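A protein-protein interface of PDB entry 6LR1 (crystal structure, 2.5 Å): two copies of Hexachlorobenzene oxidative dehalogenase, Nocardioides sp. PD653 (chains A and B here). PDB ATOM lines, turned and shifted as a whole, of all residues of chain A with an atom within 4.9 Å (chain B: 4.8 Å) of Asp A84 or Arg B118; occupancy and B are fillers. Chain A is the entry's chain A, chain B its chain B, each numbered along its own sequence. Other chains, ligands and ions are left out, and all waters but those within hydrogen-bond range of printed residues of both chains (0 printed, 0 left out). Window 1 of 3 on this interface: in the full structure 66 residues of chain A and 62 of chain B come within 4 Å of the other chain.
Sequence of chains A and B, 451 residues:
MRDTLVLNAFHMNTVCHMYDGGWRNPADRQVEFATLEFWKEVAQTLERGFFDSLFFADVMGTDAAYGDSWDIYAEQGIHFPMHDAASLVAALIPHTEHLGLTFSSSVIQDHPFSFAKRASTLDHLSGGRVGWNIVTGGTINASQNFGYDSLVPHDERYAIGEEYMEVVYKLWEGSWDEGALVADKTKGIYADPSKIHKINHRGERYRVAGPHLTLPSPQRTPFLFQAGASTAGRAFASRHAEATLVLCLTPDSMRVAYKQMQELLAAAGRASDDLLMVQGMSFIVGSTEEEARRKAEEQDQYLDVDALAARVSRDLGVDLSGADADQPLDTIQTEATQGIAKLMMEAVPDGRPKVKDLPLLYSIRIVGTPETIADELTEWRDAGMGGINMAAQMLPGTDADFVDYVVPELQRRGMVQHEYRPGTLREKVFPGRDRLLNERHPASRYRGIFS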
ATOM      1  N   ASN A  13     -16.199   5.604  -8.840  1.00  0.00           N
ATOM      2  CA  ASN A  13     -16.580   7.049  -8.809  1.00  0.00           C
ATOM      3  C   ASN A  13     -16.568   7.646  -7.393  1.00  0.00           C
ATOM      4  O   ASN A  13     -17.627   8.022  -6.825  1.00  0.00           O
ATOM      5  CB  ASN A  13     -17.953   7.272  -9.470  1.00  0.00           C
ATOM      6  CG  ASN A  13     -18.173   8.713  -9.941  1.00  0.00           C
ATOM      7  OD1 ASN A  13     -17.347   9.591  -9.700  1.00  0.00           O
ATOM      8  ND2 ASN A  13     -19.310   8.948 -10.643  1.00  0.00           N
ATOM      9  N   ASP A  58     -18.919   0.230  -8.215  1.00  0.00           N
ATOM     10  CA  ASP A  58     -19.935   1.015  -7.540  1.00  0.00           C
ATOM     11  C   ASP A  58     -20.553   0.234  -6.383  1.00  0.00           C
ATOM     12  O   ASP A  58     -20.530  -0.991  -6.372  1.00  0.00           O
ATOM     13  CB  ASP A  58     -21.019   1.389  -8.555  1.00  0.00           C
ATOM     14  CG  ASP A  58     -21.718   2.689  -8.223  1.00  0.00           C
ATOM     15  OD1 ASP A  58     -21.467   3.252  -7.143  1.00  0.00           O
ATOM     16  OD2 ASP A  58     -22.522   3.147  -9.053  1.00  0.00           O
ATOM     17  N   MET A  82     -20.151   8.282  -2.670  1.00  0.00           N
ATOM     18  CA  MET A  82     -20.184   7.392  -3.834  1.00  0.00           C
ATOM     19  C   MET A  82     -21.181   7.900  -4.868  1.00  0.00           C
ATOM     20  O   MET A  82     -22.388   7.975  -4.626  1.00  0.00           O
ATOM     21  CB  MET A  82     -20.575   5.966  -3.435  1.00  0.00           C
ATOM     22  CG  MET A  82     -20.467   4.958  -4.560  1.00  0.00           C
ATOM     23  SD  MET A  82     -18.801   4.645  -5.144  1.00  0.00           S
ATOM     24  CE  MET A  82     -17.873   4.520  -3.608  1.00  0.00           C
ATOM     25  N   HIS A  83     -20.647   8.230  -6.030  1.00  0.00           N
ATOM     26  CA  HIS A  83     -21.454   8.677  -7.127  1.00  0.00           C
ATOM     27  C   HIS A  83     -21.684   7.528  -8.161  1.00  0.00           C
ATOM     28  O   HIS A  83     -20.890   6.638  -8.344  1.00  0.00           O
ATOM     29  CB  HIS A  83     -20.820   9.916  -7.754  1.00  0.00           C
ATOM     30  CG  HIS A  83     -20.650  11.062  -6.800  1.00  0.00           C
ATOM     31  ND1 HIS A  83     -20.437  12.355  -7.225  1.00  0.00           N
ATOM     32  CD2 HIS A  83     -20.640  11.119  -5.448  1.00  0.00           C
ATOM     33  CE1 HIS A  83     -20.331  13.161  -6.186  1.00  0.00           C
ATOM     34  NE2 HIS A  83     -20.432  12.432  -5.097  1.00  0.00           N
ATOM     35  N   ASP A  84     -22.839   7.557  -8.758  1.00  0.00           N
ATOM     36  CA  ASP A  84     -23.219   6.707  -9.855  1.00  0.00           C
ATOM     37  C   ASP A  84     -22.175   6.414 -10.954  1.00  0.00           C
ATOM     38  O   ASP A  84     -21.671   7.348 -11.651  1.00  0.00           O
ATOM     39  CB  ASP A  84     -24.417   7.368 -10.525  1.00  0.00           C
ATOM     40  CG  ASP A  84     -25.048   6.498 -11.548  1.00  0.00           C
ATOM     41  OD1 ASP A  84     -25.180   5.288 -11.301  1.00  0.00           O
ATOM     42  OD2 ASP A  84     -25.462   7.038 -12.582  1.00  0.00           O
ATOM     43  N   ALA A  85     -21.883   5.128 -11.136  1.00  0.00           N
ATOM     44  CA  ALA A  85     -20.977   4.719 -12.205  1.00  0.00           C
ATOM     45  C   ALA A  85     -21.585   4.910 -13.662  1.00  0.00           C
ATOM     46  O   ALA A  85     -20.902   5.417 -14.533  1.00  0.00           O
ATOM     47  CB  ALA A  85     -20.484   3.325 -11.973  1.00  0.00           C
ATOM     48  N   ALA A  86     -22.858   4.608 -13.880  1.00  0.00           N
ATOM     49  CA  ALA A  86     -23.396   4.612 -15.241  1.00  0.00           C
ATOM     50  C   ALA A  86     -23.440   6.022 -15.857  1.00  0.00           C
ATOM     51  O   ALA A  86     -23.160   6.214 -17.022  1.00  0.00           O
ATOM     52  CB  ALA A  86     -24.798   4.011 -15.263  1.00  0.00           C
ATOM     53  N   SER A  87     -23.773   7.000 -15.050  1.00  0.00           N
ATOM     54  CA  SER A  87     -23.780   8.368 -15.510  1.00  0.00           C
ATOM     55  C   SER A  87     -22.393   8.828 -15.990  1.00  0.00           C
ATOM     56  O   SER A  87     -22.265   9.413 -17.040  1.00  0.00           O
ATOM     57  CB  SER A  87     -24.303   9.269 -14.402  1.00  0.00           C
ATOM     58  OG  SER A  87     -25.646   8.916 -14.136  1.00  0.00           O
ATOM     59  N   LEU A  88     -21.365   8.544 -15.197  1.00  0.00           N
ATOM     60  CA  LEU A  88     -19.981   8.871 -15.579  1.00  0.00           C
ATOM     61  C   LEU A  88     -19.584   8.143 -16.877  1.00  0.00           C
ATOM     62  O   LEU A  88     -19.081   8.728 -17.765  1.00  0.00           O
ATOM     63  CB  LEU A  88     -19.017   8.527 -14.446  1.00  0.00           C
ATOM     64  CG  LEU A  88     -17.516   8.756 -14.681  1.00  0.00           C
ATOM     65  CD1 LEU A  88     -17.281  10.202 -14.982  1.00  0.00           C
ATOM     66  CD2 LEU A  88     -16.720   8.370 -13.473  1.00  0.00           C
ATOM     67  N   ARG A 118     -31.381   0.867 -20.116  1.00  0.00           N
ATOM     68  CA  ARG A 118     -30.223   1.688 -19.976  1.00  0.00           C
ATOM     69  C   ARG A 118     -29.002   1.094 -20.714  1.00  0.00           C
ATOM     70  O   ARG A 118     -28.434   1.740 -21.588  1.00  0.00           O
ATOM     71  CB  ARG A 118     -29.930   1.985 -18.511  1.00  0.00           C
ATOM     72  CG  ARG A 118     -28.656   2.854 -18.276  1.00  0.00           C
ATOM     73  CD  ARG A 118     -28.248   3.034 -16.812  1.00  0.00           C
ATOM     74  NE  ARG A 118     -29.333   2.592 -15.934  1.00  0.00           N
ATOM     75  CZ  ARG A 118     -30.497   3.236 -15.740  1.00  0.00           C
ATOM     76  NH1 ARG A 118     -30.751   4.428 -16.336  1.00  0.00           N
ATOM     77  NH2 ARG A 118     -31.408   2.687 -14.915  1.00  0.00           N
ATOM     78  N   ALA B  86     -32.095   9.398 -19.530  1.00  0.00           N
ATOM     79  CA  ALA B  86     -30.979   9.884 -18.685  1.00  0.00           C
ATOM     80  C   ALA B  86     -29.604   9.569 -19.302  1.00  0.00           C
ATOM     81  O   ALA B  86     -28.719  10.370 -19.179  1.00  0.00           O
ATOM     82  CB  ALA B  86     -31.056   9.314 -17.279  1.00  0.00           C
ATOM     83  N   ASP B 110     -37.562   3.441 -11.268  1.00  0.00           N
ATOM     84  CA  ASP B 110     -36.380   3.509 -10.460  1.00  0.00           C
ATOM     85  C   ASP B 110     -36.746   3.791  -9.022  1.00  0.00           C
ATOM     86  O   ASP B 110     -37.372   4.815  -8.755  1.00  0.00           O
ATOM     87  CB  ASP B 110     -35.464   4.613 -11.013  1.00  0.00           C
ATOM     88  CG  ASP B 110     -33.977   4.346 -10.762  1.00  0.00           C
ATOM     89  OD1 ASP B 110     -33.589   3.320 -10.152  1.00  0.00           O
ATOM     90  OD2 ASP B 110     -33.173   5.192 -11.203  1.00  0.00           O
ATOM     91  N   SER B 114     -31.982   4.862  -5.488  1.00  0.00           N
ATOM     92  CA  SER B 114     -31.230   4.728  -6.742  1.00  0.00           C
ATOM     93  C   SER B 114     -31.333   5.963  -7.644  1.00  0.00           C
ATOM     94  O   SER B 114     -30.339   6.492  -8.091  1.00  0.00           O
ATOM     95  CB  SER B 114     -31.680   3.481  -7.502  1.00  0.00           C
ATOM     96  OG  SER B 114     -31.426   3.603  -8.894  1.00  0.00           O
ATOM     97  N   PHE B 115     -32.550   6.446  -7.901  1.00  0.00           N
ATOM     98  CA  PHE B 115     -32.730   7.667  -8.737  1.00  0.00           C
ATOM     99  C   PHE B 115     -32.058   8.891  -8.153  1.00  0.00           C
ATOM    100  O   PHE B 115     -31.622   9.749  -8.914  1.00  0.00           O
ATOM    101  CB  PHE B 115     -34.173   8.066  -8.891  1.00  0.00           C
ATOM    102  CG  PHE B 115     -34.350   9.288  -9.767  1.00  0.00           C
ATOM    103  CD1 PHE B 115     -34.173   9.195 -11.131  1.00  0.00           C
ATOM    104  CD2 PHE B 115     -34.658  10.528  -9.226  1.00  0.00           C
ATOM    105  CE1 PHE B 115     -34.360  10.281 -11.944  1.00  0.00           C
ATOM    106  CE2 PHE B 115     -34.823  11.641 -10.050  1.00  0.00           C
ATOM    107  CZ  PHE B 115     -34.672  11.511 -11.409  1.00  0.00           C
ATOM    108  N   ALA B 116     -32.041   8.980  -6.813  1.00  0.00           N
ATOM    109  CA  ALA B 116     -31.509  10.140  -6.106  1.00  0.00           C
ATOM    110  C   ALA B 116     -30.061  10.179  -6.359  1.00  0.00           C
ATOM    111  O   ALA B 116     -29.515  11.217  -6.523  1.00  0.00           O
ATOM    112  CB  ALA B 116     -31.779  10.063  -4.602  1.00  0.00           C
ATOM    113  N   LYS B 117     -29.425   9.026  -6.395  1.00  0.00           N
ATOM    114  CA  LYS B 117     -27.964   8.965  -6.575  1.00  0.00           C
ATOM    115  C   LYS B 117     -27.602   9.323  -8.021  1.00  0.00           C
ATOM    116  O   LYS B 117     -26.689  10.137  -8.225  1.00  0.00           O
ATOM    117  CB  LYS B 117     -27.413   7.624  -6.096  1.00  0.00           C
ATOM    118  CG  LYS B 117     -25.910   7.412  -6.272  1.00  0.00           C
ATOM    119  CD  LYS B 117     -25.552   5.918  -6.184  1.00  0.00           C
ATOM    120  CE  LYS B 117     -24.084   5.684  -5.941  1.00  0.00           C
ATOM    121  NZ  LYS B 117     -23.803   4.252  -6.279  1.00  0.00           N
ATOM    122  N   ARG B 118     -28.368   8.835  -8.999  1.00  0.00           N
ATOM    123  CA  ARG B 118     -28.172   9.255 -10.409  1.00  0.00           C
ATOM    124  C   ARG B 118     -28.375  10.792 -10.687  1.00  0.00           C
ATOM    125  O   ARG B 118     -27.474  11.434 -11.197  1.00  0.00           O
ATOM    126  CB  ARG B 118     -29.030   8.391 -11.359  1.00  0.00           C
ATOM    127  CG  ARG B 118     -28.893   8.738 -12.881  1.00  0.00           C
ATOM    128  CD  ARG B 118     -29.985   8.091 -13.742  1.00  0.00           C
ATOM    129  NE  ARG B 118     -30.619   6.987 -13.031  1.00  0.00           N
ATOM    130  CZ  ARG B 118     -30.035   5.829 -12.717  1.00  0.00           C
ATOM    131  NH1 ARG B 118     -28.769   5.534 -13.091  1.00  0.00           N
ATOM    132  NH2 ARG B 118     -30.736   4.931 -12.028  1.00  0.00           N
ATOM    133  N   ALA B 119     -29.523  11.369 -10.342  1.00  0.00           N
ATOM    134  CA  ALA B 119     -29.684  12.811 -10.466  1.00  0.00           C
ATOM    135  C   ALA B 119     -28.559  13.589  -9.823  1.00  0.00           C
ATOM    136  O   ALA B 119     -28.000  14.470 -10.450  1.00  0.00           O
ATOM    137  CB  ALA B 119     -31.004  13.276  -9.897  1.00  0.00           C
ATOM    138  N   SER B 120     -28.233  13.286  -8.570  1.00  0.00           N
ATOM    139  CA  SER B 120     -27.112  13.941  -7.863  1.00  0.00           C
ATOM    140  C   SER B 120     -25.818  13.884  -8.679  1.00  0.00           C
ATOM    141  O   SER B 120     -25.185  14.896  -8.917  1.00  0.00           O
ATOM    142  CB  SER B 120     -26.897  13.280  -6.510  1.00  0.00           C
ATOM    143  OG  SER B 120     -27.985  13.573  -5.632  1.00  0.00           O
ATOM    144  N   THR B 121     -25.468  12.693  -9.149  1.00  0.00           N
ATOM    145  CA  THR B 121     -24.308  12.532 -10.012  1.00  0.00           C
ATOM    146  C   THR B 121     -24.384  13.414 -11.266  1.00  0.00           C
ATOM    147  O   THR B 121     -23.509  14.157 -11.525  1.00  0.00           O
ATOM    148  CB  THR B 121     -24.141  11.051 -10.430  1.00  0.00           C
ATOM    149  OG1 THR B 121     -24.271  10.230  -9.272  1.00  0.00           O
ATOM    150  CG2 THR B 121     -22.760  10.793 -11.131  1.00  0.00           C
ATOM    151  N   LEU B 122     -25.426  13.337 -12.042  1.00  0.00           N
ATOM    152  CA  LEU B 122     -25.530  14.142 -13.233  1.00  0.00           C
ATOM    153  C   LEU B 122     -25.549  15.624 -12.961  1.00  0.00           C
ATOM    154  O   LEU B 122     -24.954  16.396 -13.705  1.00  0.00           O
ATOM    155  CB  LEU B 122     -26.781  13.777 -14.021  1.00  0.00           C
ATOM    156  CG  LEU B 122     -26.796  12.379 -14.630  1.00  0.00           C
ATOM    157  CD1 LEU B 122     -28.214  12.001 -14.998  1.00  0.00           C
ATOM    158  CD2 LEU B 122     -25.975  12.314 -15.863  1.00  0.00           C
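Of chain B, only Lys B117, Arg B118 and Thr B121 come within 4 Å of Asp A84. Of chain A, only Asp A84, Ser A87 and Arg A118 come within 4 Å of Arg B118. Of the printed residues of chain A, Leu B122 touches Ser A87 (3.7 Å). Of the printed residues of chain B, Asp A58 touches Lys B117 (2.7 Å).
Arg B118 touches its own counterpart, Arg A118. Of the 12 pairs that touch across the chains among the printed residues, 1 has its exchanged pair printed and touching as well.
The backbone carbonyl oxygen (O) of Asp A84 sits at hydrogen-bond distance from the side-chain amide nitrogen (ND2) of Asn A13 (3.0 Å). OD2 of Asp A58 is in hydrogen-bond range of N of Ala A85 (2.9 Å). OD2 of Asp A84 is in hydrogen-bond range of OG of Ser A87, at 2.4 Å. The guanidinium group of Arg B118 is in salt-bridge range of the side-chain carboxylate of Asp B110 (2.6 Å). The side-chain hydroxyl (OG) of Ser B114 sits at hydrogen-bond distance from the guanidinium group (NH2) of Arg B118, at 3.5 Å. O of Lys B117 is in hydrogen-bond range of OG1 of Thr B121.
The side-chain amino group (NZ) of Lys B117 is in salt-bridge range of the side-chain carboxylate (OD1) of Asp A58 (2.7 Å). The side-chain carboxylate (OD2) of Asp A84 is in salt-bridge range of the guanidinium group (NH1) of Arg B118. OG1 of Thr B121 sits at hydrogen-bond distance from N of Asp A84, at 3.1 Å.
Of the 11 printed residues of chain B, 4 touch a printed residue of chain A. Hydrophobic or aromatic side chains of chain B that line the printed part of chain A: Leu B122. Along chain B the printed residues that touch a printed residue of chain A span positions 117 to 122. Of the 10 printed residues of chain A, 7 touch a printed residue of chain B. Printed residues of chain A that touch a printed residue of chain B: Asn A13, Asp A58, Met A82, His A83, Asp A84, Ser A87 and Arg A118. Hydrophobic or aromatic side chains of chain A within 4 Å of the printed part of chain B: Met A82 and His A83. Among the printed residues, 12 pairs touch across the chains. Among the printed residues, Asp or Glu carboxylates within 4 Å of a Lys or Arg side-chain nitrogen of the other chain: Asp A58 with Lys B117 and Asp A84 with Arg B118.
Asn A13 touches Thr B121. Met A82 touches Lys B117 (O to CE, 3.1 Å). C of His A83 touches CE of Lys B117 (3.8 Å). His A83 touches Thr B121. Asp A84 touches Lys B117 (N to CE, 3.6 Å). Ser A87 touches Arg B118. CB of Ser A87 touches CG2 of Thr B121, at 3.9 Å. Leu B122 touches Ser A87. NH2 of Arg B118 touches NH2 of Arg A118, at 3.7 Å.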
